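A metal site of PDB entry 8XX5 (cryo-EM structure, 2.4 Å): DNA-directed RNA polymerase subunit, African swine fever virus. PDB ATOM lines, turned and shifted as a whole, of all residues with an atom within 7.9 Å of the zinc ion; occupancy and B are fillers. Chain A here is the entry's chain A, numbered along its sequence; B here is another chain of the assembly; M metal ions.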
ATOM      1  N   ILE A  98      17.468  -0.363  -2.254  1.00  0.00           N
ATOM      2  CA  ILE A  98      17.453  -0.772  -3.651  1.00  0.00           C
ATOM      3  C   ILE A  98      17.857   0.421  -4.521  1.00  0.00           C
ATOM      4  O   ILE A  98      17.608   1.569  -4.168  1.00  0.00           O
ATOM      5  CB  ILE A  98      16.079  -1.343  -4.079  1.00  0.00           C
ATOM      6  CG1 ILE A  98      15.038  -0.231  -4.270  1.00  0.00           C
ATOM      7  CG2 ILE A  98      15.586  -2.385  -3.092  1.00  0.00           C
ATOM      8  CD1 ILE A  98      14.792   0.100  -5.719  1.00  0.00           C
ATOM      9  N   CYS A  99      18.495   0.120  -5.649  1.00  0.00           N
ATOM     10  CA  CYS A  99      18.985   1.167  -6.542  1.00  0.00           C
ATOM     11  C   CYS A  99      17.820   1.850  -7.251  1.00  0.00           C
ATOM     12  O   CYS A  99      16.954   1.183  -7.829  1.00  0.00           O
ATOM     13  CB  CYS A  99      19.954   0.571  -7.563  1.00  0.00           C
ATOM     14  SG  CYS A  99      20.268   1.626  -8.983  1.00  0.00           S
ATOM     15  N   LEU A 100      17.808   3.179  -7.214  1.00  0.00           N
ATOM     16  CA  LEU A 100      16.721   3.965  -7.781  1.00  0.00           C
ATOM     17  C   LEU A 100      16.766   4.057  -9.301  1.00  0.00           C
ATOM     18  O   LEU A 100      15.965   4.770  -9.891  1.00  0.00           O
ATOM     19  CB  LEU A 100      16.719   5.371  -7.186  1.00  0.00           C
ATOM     20  CG  LEU A 100      16.843   5.516  -5.668  1.00  0.00           C
ATOM     21  CD1 LEU A 100      16.482   6.931  -5.254  1.00  0.00           C
ATOM     22  CD2 LEU A 100      15.972   4.517  -4.933  1.00  0.00           C
ATOM     23  N   ASN A 101      17.703   3.350  -9.947  1.00  0.00           N
ATOM     24  CA  ASN A 101      17.850   3.380 -11.396  1.00  0.00           C
ATOM     25  C   ASN A 101      17.406   2.079 -12.054  1.00  0.00           C
ATOM     26  O   ASN A 101      16.641   2.106 -13.019  1.00  0.00           O
ATOM     27  CB  ASN A 101      19.302   3.691 -11.774  1.00  0.00           C
ATOM     28  CG  ASN A 101      19.436   4.251 -13.171  1.00  0.00           C
ATOM     29  OD1 ASN A 101      19.857   3.557 -14.100  1.00  0.00           O
ATOM     30  ND2 ASN A 101      19.066   5.515 -13.325  1.00  0.00           N
ATOM     31  N   CYS A 102      17.883   0.938 -11.560  1.00  0.00           N
ATOM     32  CA  CYS A 102      17.522  -0.356 -12.126  1.00  0.00           C
ATOM     33  C   CYS A 102      16.747  -1.239 -11.151  1.00  0.00           C
ATOM     34  O   CYS A 102      16.330  -2.339 -11.547  1.00  0.00           O
ATOM     35  CB  CYS A 102      18.781  -1.091 -12.591  1.00  0.00           C
ATOM     36  SG  CYS A 102      19.980  -1.419 -11.293  1.00  0.00           S
ATOM     37  N   GLY A 103      16.548  -0.806  -9.915  1.00  0.00           N
ATOM     38  CA  GLY A 103      15.805  -1.576  -8.942  1.00  0.00           C
ATOM     39  C   GLY A 103      16.587  -2.681  -8.252  1.00  0.00           C
ATOM     40  O   GLY A 103      16.010  -3.383  -7.414  1.00  0.00           O
ATOM     41  N   ALA A 104      17.858  -2.851  -8.574  1.00  0.00           N
ATOM     42  CA  ALA A 104      18.657  -3.868  -7.915  1.00  0.00           C
ATOM     43  C   ALA A 104      18.952  -3.443  -6.468  1.00  0.00           C
ATOM     44  O   ALA A 104      18.997  -2.248  -6.162  1.00  0.00           O
ATOM     45  CB  ALA A 104      19.963  -4.096  -8.672  1.00  0.00           C
ATOM     46  N   PRO A 105      19.147  -4.405  -5.567  1.00  0.00           N
ATOM     47  CA  PRO A 105      19.470  -4.058  -4.177  1.00  0.00           C
ATOM     48  C   PRO A 105      20.904  -3.567  -4.057  1.00  0.00           C
ATOM     49  O   PRO A 105      21.842  -4.264  -4.442  1.00  0.00           O
ATOM     50  CB  PRO A 105      19.248  -5.373  -3.418  1.00  0.00           C
ATOM     51  CG  PRO A 105      19.470  -6.427  -4.451  1.00  0.00           C
ATOM     52  CD  PRO A 105      18.977  -5.855  -5.753  1.00  0.00           C
ATOM     53  N   ILE A 106      21.069  -2.350  -3.533  1.00  0.00           N
ATOM     54  CA  ILE A 106      22.405  -1.808  -3.314  1.00  0.00           C
ATOM     55  C   ILE A 106      23.120  -2.529  -2.186  1.00  0.00           C
ATOM     56  O   ILE A 106      24.355  -2.528  -2.145  1.00  0.00           O
ATOM     57  CB  ILE A 106      22.341  -0.297  -3.040  1.00  0.00           C
ATOM     58  CG1 ILE A 106      21.620  -0.033  -1.711  1.00  0.00           C
ATOM     59  CG2 ILE A 106      21.665   0.432  -4.188  1.00  0.00           C
ATOM     60  CD1 ILE A 106      21.139   1.380  -1.555  1.00  0.00           C
ATOM     61  N   GLN A 133      27.754   2.504  -4.851  1.00  0.00           N
ATOM     62  CA  GLN A 133      27.722   2.362  -6.298  1.00  0.00           C
ATOM     63  C   GLN A 133      27.030   1.049  -6.651  1.00  0.00           C
ATOM     64  O   GLN A 133      27.398  -0.017  -6.129  1.00  0.00           O
ATOM     65  CB  GLN A 133      29.137   2.382  -6.886  1.00  0.00           C
ATOM     66  CG  GLN A 133      29.188   2.825  -8.340  1.00  0.00           C
ATOM     67  CD  GLN A 133      30.330   2.190  -9.105  1.00  0.00           C
ATOM     68  OE1 GLN A 133      31.367   2.820  -9.332  1.00  0.00           O
ATOM     69  NE2 GLN A 133      30.154   0.933  -9.499  1.00  0.00           N
ATOM     70  N   CYS A 134      26.036   1.134  -7.520  1.00  0.00           N
ATOM     71  CA  CYS A 134      25.361  -0.063  -8.007  1.00  0.00           C
ATOM     72  C   CYS A 134      26.314  -0.900  -8.842  1.00  0.00           C
ATOM     73  O   CYS A 134      27.104  -0.368  -9.628  1.00  0.00           O
ATOM     74  CB  CYS A 134      24.131   0.317  -8.824  1.00  0.00           C
ATOM     75  SG  CYS A 134      23.029  -1.056  -9.218  1.00  0.00           S
ATOM     76  N   TYR A 135      26.248  -2.216  -8.669  1.00  0.00           N
ATOM     77  CA  TYR A 135      27.089  -3.118  -9.440  1.00  0.00           C
ATOM     78  C   TYR A 135      26.439  -3.557 -10.747  1.00  0.00           C
ATOM     79  O   TYR A 135      27.036  -4.351 -11.478  1.00  0.00           O
ATOM     80  CB  TYR A 135      27.470  -4.342  -8.595  1.00  0.00           C
ATOM     81  CG  TYR A 135      26.531  -5.527  -8.729  1.00  0.00           C
ATOM     82  CD1 TYR A 135      25.233  -5.466  -8.239  1.00  0.00           C
ATOM     83  CD2 TYR A 135      26.954  -6.708  -9.310  1.00  0.00           C
ATOM     84  CE1 TYR A 135      24.377  -6.547  -8.348  1.00  0.00           C
ATOM     85  CE2 TYR A 135      26.110  -7.790  -9.428  1.00  0.00           C
ATOM     86  CZ  TYR A 135      24.823  -7.713  -8.950  1.00  0.00           C
ATOM     87  OH  TYR A 135      23.980  -8.792  -9.054  1.00  0.00           O
ATOM     88  N   VAL A 136      25.252  -3.048 -11.067  1.00  0.00           N
ATOM     89  CA  VAL A 136      24.555  -3.376 -12.301  1.00  0.00           C
ATOM     90  C   VAL A 136      24.663  -2.211 -13.267  1.00  0.00           C
ATOM     91  O   VAL A 136      25.127  -2.359 -14.402  1.00  0.00           O
ATOM     92  CB  VAL A 136      23.087  -3.746 -12.046  1.00  0.00           C
ATOM     93  CG1 VAL A 136      22.357  -3.987 -13.357  1.00  0.00           C
ATOM     94  CG2 VAL A 136      22.998  -4.962 -11.142  1.00  0.00           C
ATOM     95  N   CYS A 137      24.238  -1.029 -12.825  1.00  0.00           N
ATOM     96  CA  CYS A 137      24.189   0.154 -13.671  1.00  0.00           C
ATOM     97  C   CYS A 137      25.201   1.216 -13.271  1.00  0.00           C
ATOM     98  O   CYS A 137      25.229   2.288 -13.899  1.00  0.00           O
ATOM     99  CB  CYS A 137      22.776   0.753 -13.662  1.00  0.00           C
ATOM    100  SG  CYS A 137      22.305   1.487 -12.079  1.00  0.00           S
ATOM    101  N   LYS A 138      26.020   0.961 -12.248  1.00  0.00           N
ATOM    102  CA  LYS A 138      27.108   1.866 -11.846  1.00  0.00           C
ATOM    103  C   LYS A 138      26.588   3.241 -11.428  1.00  0.00           C
ATOM    104  O   LYS A 138      27.271   4.255 -11.614  1.00  0.00           O
ATOM    105  CB  LYS A 138      28.157   2.001 -12.954  1.00  0.00           C
ATOM    106  CG  LYS A 138      29.193   0.884 -12.980  1.00  0.00           C
ATOM    107  CD  LYS A 138      28.647  -0.378 -13.631  1.00  0.00           C
ATOM    108  CE  LYS A 138      28.099  -0.079 -15.021  1.00  0.00           C
ATOM    109  NZ  LYS A 138      27.872  -1.325 -15.802  1.00  0.00           N
ATOM    110  N   ALA A 139      25.392   3.294 -10.865  1.00  0.00           N
ATOM    111  CA  ALA A 139      24.838   4.546 -10.383  1.00  0.00           C
ATOM    112  C   ALA A 139      25.127   4.730  -8.898  1.00  0.00           C
ATOM    113  O   ALA A 139      25.399   3.770  -8.173  1.00  0.00           O
ATOM    114  CB  ALA A 139      23.316   4.605 -10.625  1.00  0.00           C
ATOM    115  N   VAL A 140      25.079   5.986  -8.452  1.00  0.00           N
ATOM    116  CA  VAL A 140      25.375   6.346  -7.077  1.00  0.00           C
ATOM    117  C   VAL A 140      24.064   6.524  -6.329  1.00  0.00           C
ATOM    118  O   VAL A 140      23.214   7.319  -6.745  1.00  0.00           O
ATOM    119  CB  VAL A 140      26.233   7.621  -7.001  1.00  0.00           C
ATOM    120  CG1 VAL A 140      26.307   8.133  -5.577  1.00  0.00           C
ATOM    121  CG2 VAL A 140      27.626   7.351  -7.552  1.00  0.00           C
ATOM    122  N   ARG A 176      10.695  -1.842 -10.271  1.00  0.00           N
ATOM    123  CA  ARG A 176      11.893  -2.519 -10.760  1.00  0.00           C
ATOM    124  C   ARG A 176      12.463  -3.509  -9.763  1.00  0.00           C
ATOM    125  O   ARG A 176      13.467  -4.160 -10.064  1.00  0.00           O
ATOM    126  CB  ARG A 176      12.960  -1.479 -11.136  1.00  0.00           C
ATOM    127  CG  ARG A 176      12.659  -0.748 -12.430  1.00  0.00           C
ATOM    128  CD  ARG A 176      13.791   0.180 -12.814  1.00  0.00           C
ATOM    129  NE  ARG A 176      13.828   1.380 -11.975  1.00  0.00           N
ATOM    130  CZ  ARG A 176      13.434   2.583 -12.375  1.00  0.00           C
ATOM    131  NH1 ARG A 176      12.970   2.797 -13.591  1.00  0.00           N
ATOM    132  NH2 ARG A 176      13.531   3.598 -11.524  1.00  0.00           N
ATOM    133  N   LEU B  51      16.662  -8.809 -13.263  1.00  0.00           N
ATOM    134  CA  LEU B  51      16.110  -7.489 -12.967  1.00  0.00           C
ATOM    135  C   LEU B  51      14.639  -7.452 -13.354  1.00  0.00           C
ATOM    136  O   LEU B  51      14.100  -8.398 -13.930  1.00  0.00           O
ATOM    137  CB  LEU B  51      16.876  -6.383 -13.711  1.00  0.00           C
ATOM    138  CG  LEU B  51      18.372  -6.229 -13.425  1.00  0.00           C
ATOM    139  CD1 LEU B  51      19.190  -6.872 -14.515  1.00  0.00           C
ATOM    140  CD2 LEU B  51      18.723  -4.762 -13.268  1.00  0.00           C
HETATM  141 ZN    ZN M   1      21.418   0.158 -10.382  1.00  0.00          ZN
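SG of Cys 102 sits close to N of Ala 104, 3.7 Å away. SG of Cys 134 sits close to N of Val 136, 3.5 Å away. The backbone NH of Cys 134 is in hydrogen-bond range of the backbone carbonyl oxygen of Ala 139 (2.8 Å). The side-chain amide oxygen of Asn 101 sits close to the side-chain sulfur of Cys 137, 3.8 Å away. The side-chain sulfur (SG) of Cys 137 sits close to the backbone NH (N) of Ala 139, 3.8 Å away. SG of Cys 99 sits close to N of Asn 101. N of Cys 99 is in hydrogen-bond range of O of Ala 104.
Within 4 Å of the zinc ion: Cys 99, Cys 102, Cys 134 and Cys 137. Along chain A the residues within 4 Å of the zinc ion span positions 99 to 137.
The zinc ion is bound by the side-chain sulfur of Cys 102 (2.3 Å), the side-chain sulfur of Cys 134 (2.3 Å), the side-chain sulfur of Cys 137 (2.3 Å) and the side-chain sulfur of Cys 99 (2.3 Å).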
